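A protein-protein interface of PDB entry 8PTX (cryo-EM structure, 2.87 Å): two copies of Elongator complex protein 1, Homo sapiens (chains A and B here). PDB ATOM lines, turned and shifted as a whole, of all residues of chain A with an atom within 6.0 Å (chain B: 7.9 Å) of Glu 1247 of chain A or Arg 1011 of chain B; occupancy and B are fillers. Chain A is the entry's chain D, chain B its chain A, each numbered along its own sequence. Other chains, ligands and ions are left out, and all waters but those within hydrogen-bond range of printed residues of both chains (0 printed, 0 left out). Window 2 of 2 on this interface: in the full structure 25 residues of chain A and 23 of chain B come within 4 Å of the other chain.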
ATOM      1  N   LYS A1110     -29.258 -19.578 -20.597  1.00  0.00           N
ATOM      2  CA  LYS A1110     -29.629 -20.970 -20.347  1.00  0.00           C
ATOM      3  C   LYS A1110     -30.588 -21.531 -21.392  1.00  0.00           C
ATOM      4  O   LYS A1110     -30.363 -22.666 -21.857  1.00  0.00           O
ATOM      5  CB  LYS A1110     -30.208 -21.099 -18.932  1.00  0.00           C
ATOM      6  CG  LYS A1110     -29.193 -20.926 -17.816  1.00  0.00           C
ATOM      7  CD  LYS A1110     -29.881 -20.893 -16.461  1.00  0.00           C
ATOM      8  CE  LYS A1110     -28.881 -20.742 -15.326  1.00  0.00           C
ATOM      9  NZ  LYS A1110     -28.211 -22.032 -15.008  1.00  0.00           N
ATOM     10  N   VAL A1242     -20.134 -25.515 -20.714  1.00  0.00           N
ATOM     11  CA  VAL A1242     -21.100 -24.505 -20.293  1.00  0.00           C
ATOM     12  C   VAL A1242     -22.359 -25.159 -19.729  1.00  0.00           C
ATOM     13  O   VAL A1242     -23.019 -24.592 -18.850  1.00  0.00           O
ATOM     14  CB  VAL A1242     -21.417 -23.538 -21.452  1.00  0.00           C
ATOM     15  CG1 VAL A1242     -22.213 -24.223 -22.546  1.00  0.00           C
ATOM     16  CG2 VAL A1242     -22.144 -22.307 -20.935  1.00  0.00           C
ATOM     17  N   LEU A1243     -22.714 -26.353 -20.212  1.00  0.00           N
ATOM     18  CA  LEU A1243     -23.826 -27.091 -19.625  1.00  0.00           C
ATOM     19  C   LEU A1243     -23.495 -27.554 -18.213  1.00  0.00           C
ATOM     20  O   LEU A1243     -24.337 -27.470 -17.312  1.00  0.00           O
ATOM     21  CB  LEU A1243     -24.186 -28.289 -20.504  1.00  0.00           C
ATOM     22  CG  LEU A1243     -25.139 -28.044 -21.672  1.00  0.00           C
ATOM     23  CD1 LEU A1243     -24.927 -29.086 -22.757  1.00  0.00           C
ATOM     24  CD2 LEU A1243     -26.578 -28.062 -21.190  1.00  0.00           C
ATOM     25  N   PHE A1244     -22.273 -28.052 -18.002  1.00  0.00           N
ATOM     26  CA  PHE A1244     -21.890 -28.502 -16.668  1.00  0.00           C
ATOM     27  C   PHE A1244     -21.903 -27.346 -15.680  1.00  0.00           C
ATOM     28  O   PHE A1244     -22.358 -27.500 -14.541  1.00  0.00           O
ATOM     29  CB  PHE A1244     -20.507 -29.160 -16.701  1.00  0.00           C
ATOM     30  CG  PHE A1244     -20.025 -29.632 -15.352  1.00  0.00           C
ATOM     31  CD1 PHE A1244     -19.401 -28.763 -14.469  1.00  0.00           C
ATOM     32  CD2 PHE A1244     -20.191 -30.953 -14.972  1.00  0.00           C
ATOM     33  CE1 PHE A1244     -18.968 -29.199 -13.233  1.00  0.00           C
ATOM     34  CE2 PHE A1244     -19.753 -31.395 -13.738  1.00  0.00           C
ATOM     35  CZ  PHE A1244     -19.139 -30.517 -12.869  1.00  0.00           C
ATOM     36  N   LEU A1245     -21.404 -26.178 -16.093  1.00  0.00           N
ATOM     37  CA  LEU A1245     -21.327 -25.050 -15.172  1.00  0.00           C
ATOM     38  C   LEU A1245     -22.698 -24.608 -14.671  1.00  0.00           C
ATOM     39  O   LEU A1245     -22.783 -23.984 -13.608  1.00  0.00           O
ATOM     40  CB  LEU A1245     -20.610 -23.873 -15.836  1.00  0.00           C
ATOM     41  CG  LEU A1245     -20.275 -22.678 -14.939  1.00  0.00           C
ATOM     42  CD1 LEU A1245     -19.403 -23.109 -13.769  1.00  0.00           C
ATOM     43  CD2 LEU A1245     -19.600 -21.570 -15.732  1.00  0.00           C
ATOM     44  N   PHE A1246     -23.769 -24.936 -15.392  1.00  0.00           N
ATOM     45  CA  PHE A1246     -25.110 -24.475 -15.057  1.00  0.00           C
ATOM     46  C   PHE A1246     -25.968 -25.574 -14.435  1.00  0.00           C
ATOM     47  O   PHE A1246     -27.195 -25.548 -14.549  1.00  0.00           O
ATOM     48  CB  PHE A1246     -25.790 -23.897 -16.297  1.00  0.00           C
ATOM     49  CG  PHE A1246     -25.294 -22.530 -16.668  1.00  0.00           C
ATOM     50  CD1 PHE A1246     -25.117 -21.561 -15.696  1.00  0.00           C
ATOM     51  CD2 PHE A1246     -24.990 -22.220 -17.980  1.00  0.00           C
ATOM     52  CE1 PHE A1246     -24.656 -20.303 -16.028  1.00  0.00           C
ATOM     53  CE2 PHE A1246     -24.526 -20.962 -18.317  1.00  0.00           C
ATOM     54  CZ  PHE A1246     -24.361 -20.004 -17.340  1.00  0.00           C
ATOM     55  N   GLU A1247     -25.330 -26.542 -13.772  1.00  0.00           N
ATOM     56  CA  GLU A1247     -26.029 -27.580 -13.008  1.00  0.00           C
ATOM     57  C   GLU A1247     -27.005 -28.365 -13.881  1.00  0.00           C
ATOM     58  O   GLU A1247     -28.122 -28.686 -13.470  1.00  0.00           O
ATOM     59  CB  GLU A1247     -26.754 -26.972 -11.806  1.00  0.00           C
ATOM     60  CG  GLU A1247     -25.833 -26.360 -10.768  1.00  0.00           C
ATOM     61  CD  GLU A1247     -26.594 -25.644  -9.671  1.00  0.00           C
ATOM     62  OE1 GLU A1247     -27.833 -25.526  -9.786  1.00  0.00           O
ATOM     63  OE2 GLU A1247     -25.956 -25.194  -8.697  1.00  0.00           O
ATOM     64  N   PHE A1248     -26.581 -28.680 -15.102  1.00  0.00           N
ATOM     65  CA  PHE A1248     -27.416 -29.386 -16.073  1.00  0.00           C
ATOM     66  C   PHE A1248     -26.730 -30.705 -16.414  1.00  0.00           C
ATOM     67  O   PHE A1248     -25.890 -30.763 -17.316  1.00  0.00           O
ATOM     68  CB  PHE A1248     -27.643 -28.526 -17.312  1.00  0.00           C
ATOM     69  CG  PHE A1248     -28.436 -27.280 -17.041  1.00  0.00           C
ATOM     70  CD1 PHE A1248     -29.372 -27.247 -16.020  1.00  0.00           C
ATOM     71  CD2 PHE A1248     -28.238 -26.138 -17.797  1.00  0.00           C
ATOM     72  CE1 PHE A1248     -30.100 -26.102 -15.764  1.00  0.00           C
ATOM     73  CE2 PHE A1248     -28.963 -24.989 -17.546  1.00  0.00           C
ATOM     74  CZ  PHE A1248     -29.896 -24.970 -16.527  1.00  0.00           C
ATOM     75  N   ASP A1249     -27.097 -31.764 -15.693  1.00  0.00           N
ATOM     76  CA  ASP A1249     -26.434 -33.057 -15.817  1.00  0.00           C
ATOM     77  C   ASP A1249     -27.004 -33.903 -16.949  1.00  0.00           C
ATOM     78  O   ASP A1249     -26.245 -34.480 -17.734  1.00  0.00           O
ATOM     79  CB  ASP A1249     -26.538 -33.822 -14.495  1.00  0.00           C
ATOM     80  CG  ASP A1249     -25.934 -33.063 -13.335  1.00  0.00           C
ATOM     81  OD1 ASP A1249     -26.445 -31.970 -13.010  1.00  0.00           O
ATOM     82  OD2 ASP A1249     -24.949 -33.558 -12.748  1.00  0.00           O
ATOM     83  N   LEU A1331     -17.862 -34.899 -15.469  1.00  0.00           N
ATOM     84  CA  LEU A1331     -19.038 -35.735 -15.251  1.00  0.00           C
ATOM     85  C   LEU A1331     -18.647 -37.141 -14.813  1.00  0.00           C
ATOM     86  O   LEU A1331     -19.191 -37.670 -13.837  1.00  0.00           O
ATOM     87  CB  LEU A1331     -19.884 -35.783 -16.523  1.00  0.00           C
ATOM     88  CG  LEU A1331     -20.796 -34.584 -16.794  1.00  0.00           C
ATOM     89  CD1 LEU A1331     -21.803 -34.913 -17.883  1.00  0.00           C
ATOM     90  CD2 LEU A1331     -21.507 -34.161 -15.520  1.00  0.00           C
ATOM     91  N   LEU B 975     -21.949 -37.522  -3.691  1.00  0.00           N
ATOM     92  CA  LEU B 975     -22.746 -36.451  -4.279  1.00  0.00           C
ATOM     93  C   LEU B 975     -24.101 -36.971  -4.740  1.00  0.00           C
ATOM     94  O   LEU B 975     -25.117 -36.278  -4.617  1.00  0.00           O
ATOM     95  CB  LEU B 975     -21.990 -35.812  -5.443  1.00  0.00           C
ATOM     96  CG  LEU B 975     -20.735 -35.015  -5.080  1.00  0.00           C
ATOM     97  CD1 LEU B 975     -20.058 -34.484  -6.332  1.00  0.00           C
ATOM     98  CD2 LEU B 975     -21.079 -33.878  -4.132  1.00  0.00           C
ATOM     99  N   PRO B 980     -28.439 -31.692  -3.784  1.00  0.00           N
ATOM    100  CA  PRO B 980     -27.520 -30.547  -3.910  1.00  0.00           C
ATOM    101  C   PRO B 980     -27.788 -29.437  -2.911  1.00  0.00           C
ATOM    102  O   PRO B 980     -26.847 -28.747  -2.497  1.00  0.00           O
ATOM    103  CB  PRO B 980     -27.749 -30.075  -5.352  1.00  0.00           C
ATOM    104  CG  PRO B 980     -28.271 -31.280  -6.065  1.00  0.00           C
ATOM    105  CD  PRO B 980     -29.107 -32.010  -5.056  1.00  0.00           C
ATOM    106  N   TYR B 985     -23.611 -31.718   0.648  1.00  0.00           N
ATOM    107  CA  TYR B 985     -23.261 -31.710  -0.767  1.00  0.00           C
ATOM    108  C   TYR B 985     -22.208 -30.650  -1.059  1.00  0.00           C
ATOM    109  O   TYR B 985     -21.260 -30.895  -1.812  1.00  0.00           O
ATOM    110  CB  TYR B 985     -24.516 -31.479  -1.608  1.00  0.00           C
ATOM    111  CG  TYR B 985     -24.331 -31.703  -3.090  1.00  0.00           C
ATOM    112  CD1 TYR B 985     -23.895 -30.678  -3.919  1.00  0.00           C
ATOM    113  CD2 TYR B 985     -24.603 -32.938  -3.662  1.00  0.00           C
ATOM    114  CE1 TYR B 985     -23.730 -30.880  -5.277  1.00  0.00           C
ATOM    115  CE2 TYR B 985     -24.441 -33.148  -5.018  1.00  0.00           C
ATOM    116  CZ  TYR B 985     -24.004 -32.116  -5.820  1.00  0.00           C
ATOM    117  OH  TYR B 985     -23.841 -32.323  -7.170  1.00  0.00           O
ATOM    118  N   GLN B 986     -22.352 -29.469  -0.454  1.00  0.00           N
ATOM    119  CA  GLN B 986     -21.355 -28.416  -0.625  1.00  0.00           C
ATOM    120  C   GLN B 986     -20.001 -28.835  -0.064  1.00  0.00           C
ATOM    121  O   GLN B 986     -18.960 -28.583  -0.683  1.00  0.00           O
ATOM    122  CB  GLN B 986     -21.841 -27.131   0.045  1.00  0.00           C
ATOM    123  CG  GLN B 986     -20.928 -25.938  -0.150  1.00  0.00           C
ATOM    124  CD  GLN B 986     -21.509 -24.667   0.433  1.00  0.00           C
ATOM    125  OE1 GLN B 986     -22.593 -24.678   1.015  1.00  0.00           O
ATOM    126  NE2 GLN B 986     -20.790 -23.563   0.278  1.00  0.00           N
ATOM    127  N   SER B 989     -18.453 -31.323  -2.345  1.00  0.00           N
ATOM    128  CA  SER B 989     -17.998 -30.630  -3.546  1.00  0.00           C
ATOM    129  C   SER B 989     -16.672 -29.921  -3.302  1.00  0.00           C
ATOM    130  O   SER B 989     -15.772 -29.968  -4.144  1.00  0.00           O
ATOM    131  CB  SER B 989     -19.059 -29.634  -4.010  1.00  0.00           C
ATOM    132  OG  SER B 989     -20.269 -30.293  -4.337  1.00  0.00           O
ATOM    133  N   PRO B1004     -11.533 -27.784 -14.489  1.00  0.00           N
ATOM    134  CA  PRO B1004     -12.752 -28.483 -14.042  1.00  0.00           C
ATOM    135  C   PRO B1004     -13.120 -28.200 -12.597  1.00  0.00           C
ATOM    136  O   PRO B1004     -14.288 -27.915 -12.296  1.00  0.00           O
ATOM    137  CB  PRO B1004     -12.396 -29.961 -14.255  1.00  0.00           C
ATOM    138  CG  PRO B1004     -11.358 -29.947 -15.314  1.00  0.00           C
ATOM    139  CD  PRO B1004     -10.539 -28.734 -15.022  1.00  0.00           C
ATOM    140  N   ALA B1005     -12.145 -28.272 -11.690  1.00  0.00           N
ATOM    141  CA  ALA B1005     -12.436 -28.039 -10.281  1.00  0.00           C
ATOM    142  C   ALA B1005     -12.813 -26.590 -10.025  1.00  0.00           C
ATOM    143  O   ALA B1005     -13.621 -26.309  -9.139  1.00  0.00           O
ATOM    144  CB  ALA B1005     -11.244 -28.441  -9.421  1.00  0.00           C
ATOM    145  N   GLY B1006     -12.240 -25.655 -10.782  1.00  0.00           N
ATOM    146  CA  GLY B1006     -12.678 -24.274 -10.675  1.00  0.00           C
ATOM    147  C   GLY B1006     -14.109 -24.088 -11.141  1.00  0.00           C
ATOM    148  O   GLY B1006     -14.886 -23.357 -10.519  1.00  0.00           O
ATOM    149  N   LEU B1007     -14.479 -24.754 -12.239  1.00  0.00           N
ATOM    150  CA  LEU B1007     -15.863 -24.707 -12.701  1.00  0.00           C
ATOM    151  C   LEU B1007     -16.806 -25.254 -11.640  1.00  0.00           C
ATOM    152  O   LEU B1007     -17.871 -24.680 -11.380  1.00  0.00           O
ATOM    153  CB  LEU B1007     -16.014 -25.501 -13.997  1.00  0.00           C
ATOM    154  CG  LEU B1007     -15.476 -24.887 -15.287  1.00  0.00           C
ATOM    155  CD1 LEU B1007     -15.212 -25.980 -16.309  1.00  0.00           C
ATOM    156  CD2 LEU B1007     -16.450 -23.860 -15.837  1.00  0.00           C
ATOM    157  N   MET B1008     -16.425 -26.362 -11.007  1.00  0.00           N
ATOM    158  CA  MET B1008     -17.308 -26.971 -10.019  1.00  0.00           C
ATOM    159  C   MET B1008     -17.306 -26.177  -8.712  1.00  0.00           C
ATOM    160  O   MET B1008     -18.306 -26.165  -7.984  1.00  0.00           O
ATOM    161  CB  MET B1008     -16.913 -28.440  -9.835  1.00  0.00           C
ATOM    162  CG  MET B1008     -17.769 -29.264  -8.885  1.00  0.00           C
ATOM    163  SD  MET B1008     -17.319 -29.064  -7.162  1.00  0.00           S
ATOM    164  CE  MET B1008     -15.778 -29.971  -7.191  1.00  0.00           C
ATOM    165  N   PHE B1009     -16.205 -25.478  -8.413  1.00  0.00           N
ATOM    166  CA  PHE B1009     -16.206 -24.513  -7.318  1.00  0.00           C
ATOM    167  C   PHE B1009     -17.192 -23.387  -7.586  1.00  0.00           C
ATOM    168  O   PHE B1009     -17.943 -22.977  -6.693  1.00  0.00           O
ATOM    169  CB  PHE B1009     -14.805 -23.929  -7.117  1.00  0.00           C
ATOM    170  CG  PHE B1009     -13.878 -24.799  -6.318  1.00  0.00           C
ATOM    171  CD1 PHE B1009     -14.333 -25.496  -5.214  1.00  0.00           C
ATOM    172  CD2 PHE B1009     -12.538 -24.893  -6.657  1.00  0.00           C
ATOM    173  CE1 PHE B1009     -13.473 -26.285  -4.476  1.00  0.00           C
ATOM    174  CE2 PHE B1009     -11.676 -25.680  -5.925  1.00  0.00           C
ATOM    175  CZ  PHE B1009     -12.142 -26.376  -4.833  1.00  0.00           C
ATOM    176  N   ALA B1010     -17.192 -22.864  -8.813  1.00  0.00           N
ATOM    177  CA  ALA B1010     -18.155 -21.829  -9.174  1.00  0.00           C
ATOM    178  C   ALA B1010     -19.578 -22.362  -9.085  1.00  0.00           C
ATOM    179  O   ALA B1010     -20.500 -21.637  -8.694  1.00  0.00           O
ATOM    180  CB  ALA B1010     -17.859 -21.303 -10.579  1.00  0.00           C
ATOM    181  N   ARG B1011     -19.774 -23.629  -9.455  1.00  0.00           N
ATOM    182  CA  ARG B1011     -21.085 -24.252  -9.309  1.00  0.00           C
ATOM    183  C   ARG B1011     -21.523 -24.280  -7.849  1.00  0.00           C
ATOM    184  O   ARG B1011     -22.627 -23.838  -7.511  1.00  0.00           O
ATOM    185  CB  ARG B1011     -21.064 -25.670  -9.880  1.00  0.00           C
ATOM    186  CG  ARG B1011     -22.349 -26.433  -9.610  1.00  0.00           C
ATOM    187  CD  ARG B1011     -22.255 -27.898 -10.005  1.00  0.00           C
ATOM    188  NE  ARG B1011     -22.366 -28.110 -11.443  1.00  0.00           N
ATOM    189  CZ  ARG B1011     -22.311 -29.301 -12.024  1.00  0.00           C
ATOM    190  NH1 ARG B1011     -22.141 -30.407 -11.319  1.00  0.00           N
ATOM    191  NH2 ARG B1011     -22.436 -29.384 -13.345  1.00  0.00           N
ATOM    192  N   CYS B1012     -20.668 -24.802  -6.965  1.00  0.00           N
ATOM    193  CA  CYS B1012     -21.052 -24.915  -5.561  1.00  0.00           C
ATOM    194  C   CYS B1012     -21.091 -23.551  -4.884  1.00  0.00           C
ATOM    195  O   CYS B1012     -22.004 -23.268  -4.101  1.00  0.00           O
ATOM    196  CB  CYS B1012     -20.100 -25.856  -4.819  1.00  0.00           C
ATOM    197  SG  CYS B1012     -18.429 -25.219  -4.573  1.00  0.00           S
ATOM    198  N   GLY B1013     -20.115 -22.692  -5.171  1.00  0.00           N
ATOM    199  CA  GLY B1013     -20.103 -21.363  -4.593  1.00  0.00           C
ATOM    200  C   GLY B1013     -18.760 -20.911  -4.057  1.00  0.00           C
ATOM    201  O   GLY B1013     -18.664 -19.849  -3.436  1.00  0.00           O
ATOM    202  N   ALA B1014     -17.712 -21.706  -4.283  1.00  0.00           N
ATOM    203  CA  ALA B1014     -16.360 -21.342  -3.858  1.00  0.00           C
ATOM    204  C   ALA B1014     -15.758 -20.425  -4.918  1.00  0.00           C
ATOM    205  O   ALA B1014     -14.941 -20.826  -5.750  1.00  0.00           O
ATOM    206  CB  ALA B1014     -15.511 -22.586  -3.632  1.00  0.00           C
ATOM    207  N   HIS B1015     -16.179 -19.159  -4.875  1.00  0.00           N
ATOM    208  CA  HIS B1015     -15.803 -18.214  -5.922  1.00  0.00           C
ATOM    209  C   HIS B1015     -14.306 -17.920  -5.908  1.00  0.00           C
ATOM    210  O   HIS B1015     -13.660 -17.918  -6.961  1.00  0.00           O
ATOM    211  CB  HIS B1015     -16.606 -16.924  -5.769  1.00  0.00           C
ATOM    212  CG  HIS B1015     -18.066 -17.081  -6.060  1.00  0.00           C
ATOM    213  ND1 HIS B1015     -18.559 -18.071  -6.883  1.00  0.00           N
ATOM    214  CD2 HIS B1015     -19.142 -16.376  -5.636  1.00  0.00           C
ATOM    215  CE1 HIS B1015     -19.873 -17.969  -6.955  1.00  0.00           C
ATOM    216  NE2 HIS B1015     -20.253 -16.948  -6.208  1.00  0.00           N
ATOM    217  N   ALA B1018     -12.377 -20.584  -7.277  1.00  0.00           N
ATOM    218  CA  ALA B1018     -12.520 -20.537  -8.727  1.00  0.00           C
ATOM    219  C   ALA B1018     -11.541 -19.544  -9.340  1.00  0.00           C
ATOM    220  O   ALA B1018     -10.914 -19.838 -10.363  1.00  0.00           O
ATOM    221  CB  ALA B1018     -13.958 -20.190  -9.108  1.00  0.00           C
ATOM    222  N   PHE B1022      -8.711 -20.864 -11.912  1.00  0.00           N
ATOM    223  CA  PHE B1022      -8.756 -20.285 -13.248  1.00  0.00           C
ATOM    224  C   PHE B1022      -7.486 -19.510 -13.568  1.00  0.00           C
ATOM    225  O   PHE B1022      -6.989 -19.576 -14.698  1.00  0.00           O
ATOM    226  CB  PHE B1022      -9.983 -19.387 -13.364  1.00  0.00           C
ATOM    227  CG  PHE B1022     -11.287 -20.133 -13.337  1.00  0.00           C
ATOM    228  CD1 PHE B1022     -11.323 -21.504 -13.531  1.00  0.00           C
ATOM    229  CD2 PHE B1022     -12.469 -19.475 -13.048  1.00  0.00           C
ATOM    230  CE1 PHE B1022     -12.520 -22.191 -13.496  1.00  0.00           C
ATOM    231  CE2 PHE B1022     -13.669 -20.157 -13.004  1.00  0.00           C
ATOM    232  CZ  PHE B1022     -13.694 -21.516 -13.229  1.00  0.00           C
ATOM    233  N   VAL B1034     -15.821 -14.926 -12.688  1.00  0.00           N
ATOM    234  CA  VAL B1034     -16.065 -15.150 -11.266  1.00  0.00           C
ATOM    235  C   VAL B1034     -15.621 -13.942 -10.447  1.00  0.00           C
ATOM    236  O   VAL B1034     -16.231 -13.611  -9.421  1.00  0.00           O
ATOM    237  CB  VAL B1034     -15.388 -16.450 -10.797  1.00  0.00           C
ATOM    238  CG1 VAL B1034     -15.823 -16.790  -9.381  1.00  0.00           C
ATOM    239  CG2 VAL B1034     -15.740 -17.589 -11.735  1.00  0.00           C
ATOM    240  N   GLN B1037     -18.437 -11.640 -10.625  1.00  0.00           N
ATOM    241  CA  GLN B1037     -19.461 -12.111  -9.695  1.00  0.00           C
ATOM    242  C   GLN B1037     -19.091 -11.811  -8.248  1.00  0.00           C
ATOM    243  O   GLN B1037     -19.973 -11.732  -7.385  1.00  0.00           O
ATOM    244  CB  GLN B1037     -19.718 -13.608  -9.880  1.00  0.00           C
ATOM    245  CG  GLN B1037     -20.015 -14.020 -11.310  1.00  0.00           C
ATOM    246  CD  GLN B1037     -19.976 -15.522 -11.505  1.00  0.00           C
ATOM    247  OE1 GLN B1037     -19.147 -16.216 -10.917  1.00  0.00           O
ATOM    248  NE2 GLN B1037     -20.877 -16.033 -12.336  1.00  0.00           N
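Of chain B, only Arg 1011 comes within 4 Å of Glu 1247 of chain A. Arg 1011 of chain B touches just these residues of chain A: Phe 1244 (2.2 Å) and Glu 1247 (3.7 Å). Printed residues of chain A within 4 Å of Ala 1010 of chain B: Leu 1245. Printed residues of chain A within 4 Å of Leu 1007 of chain B: Leu 1245.
Among the printed residues, merely in contact across the chains: Leu 1245 of chain A with Leu 1007 of chain B, Leu 1245 of chain A with Ala 1010 of chain B and Glu 1247 of chain A with Arg 1011 of chain B.
No position is printed for both chains. Of the 4 pairs that touch across the chains among the printed residues, none has its exchanged pair printed and touching as well.
NE of Arg 1011 of chain B lies close to O of Phe 1244 of chain A (3.2 Å).
Of the 10 printed residues of chain A, 3 touch a printed residue of chain B. Of the 21 printed residues of chain B, 3 touch a printed residue of chain A. Printed residues of chain B that touch a printed residue of chain A: Leu 1007, Ala 1010 and Arg 1011. Hydrophobic or aromatic side chains of chain B that line the printed part of chain A: Leu 1007 and Ala 1010. Among the printed residues, 4 pairs touch across the chains.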
